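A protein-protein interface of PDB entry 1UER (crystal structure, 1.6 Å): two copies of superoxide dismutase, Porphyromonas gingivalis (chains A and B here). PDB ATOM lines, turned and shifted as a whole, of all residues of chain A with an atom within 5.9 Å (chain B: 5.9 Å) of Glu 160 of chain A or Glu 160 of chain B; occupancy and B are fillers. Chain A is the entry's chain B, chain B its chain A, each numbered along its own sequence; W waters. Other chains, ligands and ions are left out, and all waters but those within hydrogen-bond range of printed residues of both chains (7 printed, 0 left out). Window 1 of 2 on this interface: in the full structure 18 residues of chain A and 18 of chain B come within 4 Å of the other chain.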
ATOM      1  N   HIS A  31     -25.104 -24.717 -27.234  1.00  0.00           N
ATOM      2  CA  HIS A  31     -25.969 -23.974 -26.315  1.00  0.00           C
ATOM      3  C   HIS A  31     -27.245 -24.745 -25.907  1.00  0.00           C
ATOM      4  O   HIS A  31     -27.550 -24.873 -24.720  1.00  0.00           O
ATOM      5  CB  HIS A  31     -26.363 -22.631 -26.922  1.00  0.00           C
ATOM      6  CG  HIS A  31     -25.208 -21.682 -27.077  1.00  0.00           C
ATOM      7  ND1 HIS A  31     -24.881 -20.750 -26.112  1.00  0.00           N
ATOM      8  CD2 HIS A  31     -24.295 -21.534 -28.066  1.00  0.00           C
ATOM      9  CE1 HIS A  31     -23.818 -20.068 -26.508  1.00  0.00           C
ATOM     10  NE2 HIS A  31     -23.443 -20.522 -27.688  1.00  0.00           N
ATOM     11  N   SER A 121     -29.769  -9.642 -23.449  1.00  0.00           N
ATOM     12  CA  SER A 121     -30.193 -10.901 -24.079  1.00  0.00           C
ATOM     13  C   SER A 121     -31.701 -11.096 -23.989  1.00  0.00           C
ATOM     14  O   SER A 121     -32.323 -10.640 -23.029  1.00  0.00           O
ATOM     15  CB  SER A 121     -29.534 -12.094 -23.385  1.00  0.00           C
ATOM     16  OG  SER A 121     -28.115 -12.001 -23.419  1.00  0.00           O
ATOM     17  N   ASP A 157     -34.487 -14.876 -31.719  1.00  0.00           N
ATOM     18  CA  ASP A 157     -33.512 -14.900 -30.637  1.00  0.00           C
ATOM     19  C   ASP A 157     -32.558 -13.717 -30.780  1.00  0.00           C
ATOM     20  O   ASP A 157     -31.894 -13.601 -31.811  1.00  0.00           O
ATOM     21  CB  ASP A 157     -32.746 -16.233 -30.732  1.00  0.00           C
ATOM     22  CG  ASP A 157     -31.802 -16.486 -29.575  1.00  0.00           C
ATOM     23  OD1 ASP A 157     -31.714 -15.676 -28.629  1.00  0.00           O
ATOM     24  OD2 ASP A 157     -31.164 -17.558 -29.618  1.00  0.00           O
ATOM     25  N   VAL A 158     -32.507 -12.836 -29.773  1.00  0.00           N
ATOM     26  CA  VAL A 158     -31.568 -11.720 -29.842  1.00  0.00           C
ATOM     27  C   VAL A 158     -30.416 -11.854 -28.855  1.00  0.00           C
ATOM     28  O   VAL A 158     -29.698 -10.889 -28.595  1.00  0.00           O
ATOM     29  CB  VAL A 158     -32.246 -10.308 -29.755  1.00  0.00           C
ATOM     30  CG1 VAL A 158     -33.167 -10.085 -31.001  1.00  0.00           C
ATOM     31  CG2 VAL A 158     -33.048 -10.151 -28.427  1.00  0.00           C
ATOM     32  N   TRP A 159     -30.260 -13.048 -28.281  1.00  0.00           N
ATOM     33  CA  TRP A 159     -29.073 -13.324 -27.496  1.00  0.00           C
ATOM     34  C   TRP A 159     -27.951 -13.158 -28.547  1.00  0.00           C
ATOM     35  O   TRP A 159     -28.095 -13.584 -29.712  1.00  0.00           O
ATOM     36  CB  TRP A 159     -29.072 -14.768 -27.006  1.00  0.00           C
ATOM     37  CG  TRP A 159     -29.881 -14.960 -25.787  1.00  0.00           C
ATOM     38  CD1 TRP A 159     -31.232 -14.806 -25.671  1.00  0.00           C
ATOM     39  CD2 TRP A 159     -29.407 -15.407 -24.504  1.00  0.00           C
ATOM     40  NE1 TRP A 159     -31.630 -15.140 -24.380  1.00  0.00           N
ATOM     41  CE2 TRP A 159     -30.532 -15.510 -23.652  1.00  0.00           C
ATOM     42  CE3 TRP A 159     -28.141 -15.732 -23.995  1.00  0.00           C
ATOM     43  CZ2 TRP A 159     -30.430 -15.928 -22.308  1.00  0.00           C
ATOM     44  CZ3 TRP A 159     -28.035 -16.143 -22.658  1.00  0.00           C
ATOM     45  CH2 TRP A 159     -29.169 -16.242 -21.831  1.00  0.00           C
ATOM     46  N   GLU A 160     -26.831 -12.578 -28.170  1.00  0.00           N
ATOM     47  CA  GLU A 160     -25.746 -12.392 -29.149  1.00  0.00           C
ATOM     48  C   GLU A 160     -25.204 -13.682 -29.785  1.00  0.00           C
ATOM     49  O   GLU A 160     -24.784 -13.660 -30.959  1.00  0.00           O
ATOM     50  CB  GLU A 160     -24.624 -11.561 -28.518  1.00  0.00           C
ATOM     51  CG  GLU A 160     -25.061 -10.098 -28.353  1.00  0.00           C
ATOM     52  CD  GLU A 160     -24.044  -9.206 -27.656  1.00  0.00           C
ATOM     53  OE1 GLU A 160     -23.427  -9.666 -26.661  1.00  0.00           O
ATOM     54  OE2 GLU A 160     -23.877  -8.041 -28.102  1.00  0.00           O
ATOM     55  N   HIS A 161     -25.241 -14.807 -29.071  1.00  0.00           N
ATOM     56  CA  HIS A 161     -24.773 -16.058 -29.695  1.00  0.00           C
ATOM     57  C   HIS A 161     -25.575 -16.449 -30.937  1.00  0.00           C
ATOM     58  O   HIS A 161     -25.084 -17.243 -31.741  1.00  0.00           O
ATOM     59  CB  HIS A 161     -24.745 -17.230 -28.701  1.00  0.00           C
ATOM     60  CG  HIS A 161     -26.084 -17.591 -28.114  1.00  0.00           C
ATOM     61  ND1 HIS A 161     -26.319 -17.583 -26.756  1.00  0.00           N
ATOM     62  CD2 HIS A 161     -27.231 -18.022 -28.694  1.00  0.00           C
ATOM     63  CE1 HIS A 161     -27.555 -18.006 -26.520  1.00  0.00           C
ATOM     64  NE2 HIS A 161     -28.127 -18.274 -27.677  1.00  0.00           N
ATOM     65  N   ALA A 162     -26.785 -15.923 -31.095  1.00  0.00           N
ATOM     66  CA  ALA A 162     -27.601 -16.247 -32.267  1.00  0.00           C
ATOM     67  C   ALA A 162     -27.108 -15.617 -33.569  1.00  0.00           C
ATOM     68  O   ALA A 162     -27.367 -16.144 -34.654  1.00  0.00           O
ATOM     69  CB  ALA A 162     -29.076 -15.846 -32.020  1.00  0.00           C
ATOM     70  N   TYR A 163     -26.344 -14.536 -33.478  1.00  0.00           N
ATOM     71  CA  TYR A 163     -25.947 -13.843 -34.705  1.00  0.00           C
ATOM     72  C   TYR A 163     -24.532 -13.285 -34.713  1.00  0.00           C
ATOM     73  O   TYR A 163     -24.060 -12.836 -35.751  1.00  0.00           O
ATOM     74  CB  TYR A 163     -26.925 -12.690 -34.973  1.00  0.00           C
ATOM     75  CG  TYR A 163     -26.981 -11.672 -33.831  1.00  0.00           C
ATOM     76  CD1 TYR A 163     -26.028 -10.652 -33.741  1.00  0.00           C
ATOM     77  CD2 TYR A 163     -28.012 -11.725 -32.871  1.00  0.00           C
ATOM     78  CE1 TYR A 163     -26.104  -9.672 -32.692  1.00  0.00           C
ATOM     79  CE2 TYR A 163     -28.095 -10.772 -31.844  1.00  0.00           C
ATOM     80  CZ  TYR A 163     -27.142  -9.756 -31.771  1.00  0.00           C
ATOM     81  OH  TYR A 163     -27.198  -8.779 -30.783  1.00  0.00           O
ATOM     82  N   TYR A 164     -23.834 -13.339 -33.589  1.00  0.00           N
ATOM     83  CA  TYR A 164     -22.519 -12.695 -33.555  1.00  0.00           C
ATOM     84  C   TYR A 164     -21.440 -13.180 -34.521  1.00  0.00           C
ATOM     85  O   TYR A 164     -20.637 -12.358 -35.006  1.00  0.00           O
ATOM     86  CB  TYR A 164     -21.941 -12.688 -32.133  1.00  0.00           C
ATOM     87  CG  TYR A 164     -21.213 -11.401 -31.848  1.00  0.00           C
ATOM     88  CD1 TYR A 164     -21.918 -10.228 -31.590  1.00  0.00           C
ATOM     89  CD2 TYR A 164     -19.819 -11.321 -31.915  1.00  0.00           C
ATOM     90  CE1 TYR A 164     -21.273  -8.995 -31.409  1.00  0.00           C
ATOM     91  CE2 TYR A 164     -19.165 -10.079 -31.740  1.00  0.00           C
ATOM     92  CZ  TYR A 164     -19.900  -8.926 -31.490  1.00  0.00           C
ATOM     93  OH  TYR A 164     -19.321  -7.689 -31.329  1.00  0.00           O
ATOM     94  N   LEU A 165     -21.428 -14.480 -34.816  1.00  0.00           N
ATOM     95  CA  LEU A 165     -20.363 -15.011 -35.687  1.00  0.00           C
ATOM     96  C   LEU A 165     -20.438 -14.413 -37.089  1.00  0.00           C
ATOM     97  O   LEU A 165     -19.401 -14.189 -37.739  1.00  0.00           O
ATOM     98  CB  LEU A 165     -20.431 -16.555 -35.747  1.00  0.00           C
ATOM     99  CG  LEU A 165     -19.958 -17.217 -34.431  1.00  0.00           C
ATOM    100  CD1 LEU A 165     -20.077 -18.735 -34.571  1.00  0.00           C
ATOM    101  CD2 LEU A 165     -18.535 -16.805 -34.094  1.00  0.00           C
ATOM    102  N   ARG A 171     -27.163  -6.317 -35.148  1.00  0.00           N
ATOM    103  CA  ARG A 171     -28.389  -7.068 -34.842  1.00  0.00           C
ATOM    104  C   ARG A 171     -29.558  -6.732 -35.759  1.00  0.00           C
ATOM    105  O   ARG A 171     -30.278  -7.645 -36.191  1.00  0.00           O
ATOM    106  CB  ARG A 171     -28.812  -6.859 -33.359  1.00  0.00           C
ATOM    107  CG  ARG A 171     -30.016  -7.697 -32.956  1.00  0.00           C
ATOM    108  CD  ARG A 171     -30.656  -7.212 -31.657  1.00  0.00           C
ATOM    109  NE  ARG A 171     -29.876  -7.540 -30.457  1.00  0.00           N
ATOM    110  CZ  ARG A 171     -30.275  -7.222 -29.228  1.00  0.00           C
ATOM    111  NH1 ARG A 171     -31.421  -6.585 -29.053  1.00  0.00           N
ATOM    112  NH2 ARG A 171     -29.536  -7.529 -28.161  1.00  0.00           N
ATOM    113  N   HIS B  31     -19.306  -1.307 -30.354  1.00  0.00           N
ATOM    114  CA  HIS B  31     -20.190  -1.354 -29.193  1.00  0.00           C
ATOM    115  C   HIS B  31     -20.047  -0.133 -28.272  1.00  0.00           C
ATOM    116  O   HIS B  31     -21.042   0.544 -27.972  1.00  0.00           O
ATOM    117  CB  HIS B  31     -19.948  -2.642 -28.375  1.00  0.00           C
ATOM    118  CG  HIS B  31     -20.429  -3.889 -29.050  1.00  0.00           C
ATOM    119  ND1 HIS B  31     -21.716  -4.372 -28.898  1.00  0.00           N
ATOM    120  CD2 HIS B  31     -19.806  -4.743 -29.901  1.00  0.00           C
ATOM    121  CE1 HIS B  31     -21.860  -5.464 -29.632  1.00  0.00           C
ATOM    122  NE2 HIS B  31     -20.723  -5.705 -30.251  1.00  0.00           N
ATOM    123  N   SER B 121     -26.788 -11.504 -20.181  1.00  0.00           N
ATOM    124  CA  SER B 121     -25.693 -10.522 -20.315  1.00  0.00           C
ATOM    125  C   SER B 121     -25.414  -9.854 -18.968  1.00  0.00           C
ATOM    126  O   SER B 121     -26.320  -9.710 -18.149  1.00  0.00           O
ATOM    127  CB  SER B 121     -26.081  -9.399 -21.291  1.00  0.00           C
ATOM    128  OG  SER B 121     -26.464  -9.914 -22.577  1.00  0.00           O
ATOM    129  N   ASP B 157     -16.499  -8.527 -18.281  1.00  0.00           N
ATOM    130  CA  ASP B 157     -17.675  -8.422 -19.137  1.00  0.00           C
ATOM    131  C   ASP B 157     -18.085  -9.818 -19.563  1.00  0.00           C
ATOM    132  O   ASP B 157     -17.276 -10.531 -20.168  1.00  0.00           O
ATOM    133  CB  ASP B 157     -17.296  -7.602 -20.371  1.00  0.00           C
ATOM    134  CG  ASP B 157     -18.474  -7.194 -21.222  1.00  0.00           C
ATOM    135  OD1 ASP B 157     -19.612  -7.569 -20.924  1.00  0.00           O
ATOM    136  OD2 ASP B 157     -18.238  -6.469 -22.212  1.00  0.00           O
ATOM    137  N   VAL B 158     -19.314 -10.222 -19.239  1.00  0.00           N
ATOM    138  CA  VAL B 158     -19.770 -11.530 -19.663  1.00  0.00           C
ATOM    139  C   VAL B 158     -20.866 -11.426 -20.726  1.00  0.00           C
ATOM    140  O   VAL B 158     -21.510 -12.422 -21.065  1.00  0.00           O
ATOM    141  CB  VAL B 158     -20.162 -12.496 -18.483  1.00  0.00           C
ATOM    142  CG1 VAL B 158     -18.908 -12.747 -17.563  1.00  0.00           C
ATOM    143  CG2 VAL B 158     -21.295 -11.930 -17.666  1.00  0.00           C
ATOM    144  N   TRP B 159     -21.082 -10.215 -21.262  1.00  0.00           N
ATOM    145  CA  TRP B 159     -21.959 -10.097 -22.446  1.00  0.00           C
ATOM    146  C   TRP B 159     -21.236 -10.960 -23.489  1.00  0.00           C
ATOM    147  O   TRP B 159     -20.001 -10.920 -23.576  1.00  0.00           O
ATOM    148  CB  TRP B 159     -21.993  -8.669 -22.945  1.00  0.00           C
ATOM    149  CG  TRP B 159     -22.913  -7.781 -22.136  1.00  0.00           C
ATOM    150  CD1 TRP B 159     -22.801  -7.423 -20.812  1.00  0.00           C
ATOM    151  CD2 TRP B 159     -24.016  -7.050 -22.670  1.00  0.00           C
ATOM    152  NE1 TRP B 159     -23.787  -6.480 -20.505  1.00  0.00           N
ATOM    153  CE2 TRP B 159     -24.537  -6.242 -21.633  1.00  0.00           C
ATOM    154  CE3 TRP B 159     -24.613  -6.997 -23.942  1.00  0.00           C
ATOM    155  CZ2 TRP B 159     -25.634  -5.390 -21.829  1.00  0.00           C
ATOM    156  CZ3 TRP B 159     -25.718  -6.126 -24.142  1.00  0.00           C
ATOM    157  CH2 TRP B 159     -26.203  -5.338 -23.071  1.00  0.00           C
ATOM    158  N   GLU B 160     -21.978 -11.728 -24.291  1.00  0.00           N
ATOM    159  CA  GLU B 160     -21.318 -12.594 -25.281  1.00  0.00           C
ATOM    160  C   GLU B 160     -20.422 -11.884 -26.283  1.00  0.00           C
ATOM    161  O   GLU B 160     -19.438 -12.481 -26.734  1.00  0.00           O
ATOM    162  CB  GLU B 160     -22.370 -13.500 -25.998  1.00  0.00           C
ATOM    163  CG  GLU B 160     -22.918 -14.562 -25.011  1.00  0.00           C
ATOM    164  CD  GLU B 160     -24.103 -15.378 -25.536  1.00  0.00           C
ATOM    165  OE1 GLU B 160     -25.023 -14.805 -26.195  1.00  0.00           O
ATOM    166  OE2 GLU B 160     -24.099 -16.603 -25.258  1.00  0.00           O
ATOM    167  N   HIS B 161     -20.718 -10.624 -26.636  1.00  0.00           N
ATOM    168  CA  HIS B 161     -19.847  -9.919 -27.584  1.00  0.00           C
ATOM    169  C   HIS B 161     -18.418  -9.782 -27.036  1.00  0.00           C
ATOM    170  O   HIS B 161     -17.485  -9.544 -27.803  1.00  0.00           O
ATOM    171  CB  HIS B 161     -20.395  -8.521 -27.980  1.00  0.00           C
ATOM    172  CG  HIS B 161     -20.530  -7.554 -26.847  1.00  0.00           C
ATOM    173  ND1 HIS B 161     -21.742  -7.003 -26.495  1.00  0.00           N
ATOM    174  CD2 HIS B 161     -19.618  -7.025 -26.002  1.00  0.00           C
ATOM    175  CE1 HIS B 161     -21.574  -6.178 -25.474  1.00  0.00           C
ATOM    176  NE2 HIS B 161     -20.296  -6.174 -25.155  1.00  0.00           N
ATOM    177  N   ALA B 162     -18.225  -9.936 -25.724  1.00  0.00           N
ATOM    178  CA  ALA B 162     -16.874  -9.806 -25.163  1.00  0.00           C
ATOM    179  C   ALA B 162     -15.927 -10.948 -25.488  1.00  0.00           C
ATOM    180  O   ALA B 162     -14.708 -10.781 -25.496  1.00  0.00           O
ATOM    181  CB  ALA B 162     -16.941  -9.624 -23.615  1.00  0.00           C
ATOM    182  N   TYR B 163     -16.495 -12.103 -25.813  1.00  0.00           N
ATOM    183  CA  TYR B 163     -15.678 -13.284 -26.036  1.00  0.00           C
ATOM    184  C   TYR B 163     -16.152 -14.210 -27.134  1.00  0.00           C
ATOM    185  O   TYR B 163     -15.458 -15.181 -27.413  1.00  0.00           O
ATOM    186  CB  TYR B 163     -15.629 -14.125 -24.739  1.00  0.00           C
ATOM    187  CG  TYR B 163     -16.991 -14.583 -24.218  1.00  0.00           C
ATOM    188  CD1 TYR B 163     -17.619 -15.731 -24.718  1.00  0.00           C
ATOM    189  CD2 TYR B 163     -17.636 -13.876 -23.199  1.00  0.00           C
ATOM    190  CE1 TYR B 163     -18.857 -16.172 -24.220  1.00  0.00           C
ATOM    191  CE2 TYR B 163     -18.889 -14.302 -22.679  1.00  0.00           C
ATOM    192  CZ  TYR B 163     -19.486 -15.456 -23.200  1.00  0.00           C
ATOM    193  OH  TYR B 163     -20.693 -15.900 -22.699  1.00  0.00           O
ATOM    194  N   TYR B 164     -17.304 -13.954 -27.756  1.00  0.00           N
ATOM    195  CA  TYR B 164     -17.801 -14.955 -28.705  1.00  0.00           C
ATOM    196  C   TYR B 164     -16.964 -15.219 -29.963  1.00  0.00           C
ATOM    197  O   TYR B 164     -16.886 -16.355 -30.420  1.00  0.00           O
ATOM    198  CB  TYR B 164     -19.245 -14.643 -29.102  1.00  0.00           C
ATOM    199  CG  TYR B 164     -20.075 -15.898 -29.271  1.00  0.00           C
ATOM    200  CD1 TYR B 164     -20.554 -16.605 -28.159  1.00  0.00           C
ATOM    201  CD2 TYR B 164     -20.291 -16.438 -30.539  1.00  0.00           C
ATOM    202  CE1 TYR B 164     -21.238 -17.848 -28.299  1.00  0.00           C
ATOM    203  CE2 TYR B 164     -20.959 -17.666 -30.690  1.00  0.00           C
ATOM    204  CZ  TYR B 164     -21.420 -18.356 -29.577  1.00  0.00           C
ATOM    205  OH  TYR B 164     -22.056 -19.564 -29.758  1.00  0.00           O
ATOM    206  N   LEU B 165     -16.322 -14.197 -30.494  1.00  0.00           N
ATOM    207  CA  LEU B 165     -15.534 -14.385 -31.711  1.00  0.00           C
ATOM    208  C   LEU B 165     -14.371 -15.349 -31.496  1.00  0.00           C
ATOM    209  O   LEU B 165     -14.066 -16.126 -32.389  1.00  0.00           O
ATOM    210  CB  LEU B 165     -15.033 -13.031 -32.256  1.00  0.00           C
ATOM    211  CG  LEU B 165     -16.149 -12.132 -32.850  1.00  0.00           C
ATOM    212  CD1 LEU B 165     -15.560 -10.770 -33.301  1.00  0.00           C
ATOM    213  CD2 LEU B 165     -16.864 -12.817 -34.048  1.00  0.00           C
ATOM    214  N   ARG B 171     -17.380 -19.523 -22.172  1.00  0.00           N
ATOM    215  CA  ARG B 171     -17.240 -18.347 -21.313  1.00  0.00           C
ATOM    216  C   ARG B 171     -16.252 -18.613 -20.159  1.00  0.00           C
ATOM    217  O   ARG B 171     -15.448 -17.751 -19.827  1.00  0.00           O
ATOM    218  CB  ARG B 171     -18.603 -17.934 -20.761  1.00  0.00           C
ATOM    219  CG  ARG B 171     -18.551 -16.700 -19.846  1.00  0.00           C
ATOM    220  CD  ARG B 171     -19.809 -16.557 -18.996  1.00  0.00           C
ATOM    221  NE  ARG B 171     -20.943 -15.984 -19.747  1.00  0.00           N
ATOM    222  CZ  ARG B 171     -22.062 -15.612 -19.152  1.00  0.00           C
ATOM    223  NH1 ARG B 171     -22.137 -15.771 -17.831  1.00  0.00           N
ATOM    224  NH2 ARG B 171     -23.104 -15.125 -19.846  1.00  0.00           N
HETATM  225  O   HOH W   1     -26.421 -12.674 -25.354  1.00  0.00           O
HETATM  226  O   HOH W   2     -24.375  -4.885 -27.518  1.00  0.00           O
HETATM  227  O   HOH W   3     -25.399 -18.710 -23.837  1.00  0.00           O
HETATM  228  O   HOH W   4     -24.032 -19.902 -31.651  1.00  0.00           O
HETATM  229  O   HOH W   5     -29.339 -10.181 -20.658  1.00  0.00           O
HETATM  230  O   HOH W   6     -24.675 -10.780 -24.503  1.00  0.00           O
HETATM  231  O   HOH W   7     -16.931  -7.554 -29.788  1.00  0.00           O
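A ring nitrogen (NE2) of His 31 of chain B is in hydrogen-bond range of the side-chain hydroxyl (OH) of Tyr 164 of chain A (2.7 Å). The side-chain hydroxyl (OG) of Ser 121 of chain A sits at hydrogen-bond distance from the side-chain hydroxyl (OG) of Ser 121 of chain B (2.8 Å). The backbone NH (N) of Glu 160 of chain B lies within hydrogen-bond range of the side-chain carboxylate (OE1) of Glu 160 of chain A (3.5 Å). OE2 of Glu 160 of chain B lies within hydrogen-bond range of ND1 of His 161 of chain A (2.9 Å). ND1 of His 161 of chain B is in hydrogen-bond range of OE2 of Glu 160 of chain A (2.9 Å). A ring nitrogen (NE2) of His 31 of chain A is in hydrogen-bond range of the side-chain hydroxyl of Tyr 164 of chain B.
The side-chain carboxylate of Asp 157 of chain B is in hydrogen-bond range of the backbone NH of Trp 159 of chain B (3.0 Å). The backbone NH of Trp 159 of chain A is in hydrogen-bond range of the side-chain carboxylate of Asp 157 of chain A (3.0 Å).
Glu 160 of chain B touches His 31 of chain A. Glu 160 of chain B touches Trp 159 of chain A (OE1 to CE3, 3.9 Å). His 31 of chain B touches Glu 160 of chain A. Glu 160 of chain A touches Trp 159 of chain B (OE1 to CE3, 3.99 Å). His 161 of chain A touches Tyr 164 of chain B (CB to CE1, 3.6 Å). CZ of Tyr 164 of chain A touches CB of His 161 of chain B (3.6 Å). CG of Leu 165 of chain B touches CE2 of Tyr 164 of chain A, 3.8 Å away. CG of Leu 165 of chain A touches CE2 of Tyr 164 of chain B, 3.9 Å away.
Of the printed residues of chain B, Glu 160 of chain A touches His 31, Trp 159, Glu 160 and His 161. Printed residues of chain B within 4 Å of His 161 of chain A: Glu 160 (2.9 Å) and Tyr 164 (3.6 Å). Arg 171 of chain A touches none of the printed residues of chain B. Printed residues of chain A within 4 Å of His 31 of chain B: Glu 160 and Tyr 164. Of chain A, only His 31, Trp 159, Glu 160 and His 161 come within 4 Å of Glu 160 of chain B. Ala 162 of chain B touches none of the printed residues of chain A. The nearest printed residue of chain B that does not touch Glu 160 of chain A is Ser 121 of chain B (5.1 Å). The nearest printed residue of chain B that does not touch Tyr 164 of chain A is Tyr 164 of chain B (4.4 Å).
Of the 12 printed residues of chain B, 7 touch a printed residue of chain A. Of the 12 printed residues of chain A, 7 touch a printed residue of chain B. Printed residues of chain A that touch a printed residue of chain B: His 31, Ser 121, Trp 159, Glu 160, His 161, Tyr 164 and Leu 165. Among the printed residues, no Asp or Glu carboxylate lies within 4 Å of a Lys or Arg side-chain nitrogen of the other chain.
His 31 of chain A touches Glu 160 of chain B, and with the chains exchanged Glu 160 of chain A touches His 31 of chain B. His 31 of chain A touches Tyr 164 of chain B, and with the chains exchanged Tyr 164 of chain A touches His 31 of chain B. Glu 160 of chain B touches its own counterpart, Glu 160 of chain A. His 161 of chain A touches Tyr 164 of chain B, and with the chains exchanged Tyr 164 of chain A touches His 161 of chain B. Positions printed for both chains: 31, 121, 157, 158, 159, 160, 161, 162, 163, 164, 165 and 171.
Water W1 lies within hydrogen-bond range of the side-chain hydroxyl of Ser 121 of chain A (2.7 Å), the side-chain carboxylate of Glu 160 of chain B (2.7 Å) and the backbone NH of Glu 160 of chain A (2.8 Å). Water W6 lies within hydrogen-bond range of the side-chain carboxylate of Glu 160 of chain A (2.7 Å), the side-chain hydroxyl of Ser 121 of chain B (2.8 Å) and the backbone NH of Glu 160 of chain B (2.9 Å). Water W7 lies within hydrogen-bond range of OH of Tyr 164 of chain A (2.8 Å) and O of His 161 of chain B (2.9 Å). Water W3 lies within hydrogen-bond range of OE2 of Glu 160 of chain B, ND1 of His 31 of chain A and ND1 of His 161 of chain A. Water W5 bridges N of Ser 121 of chain A (2.9 Å) and N of Ser 121 of chain B (2.9 Å). Water W2 bridges a ring nitrogen (ND1) of His 31 of chain B (3.0 Å) and the side-chain carboxylate (OE2) of Glu 160 of chain A (3.2 Å).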
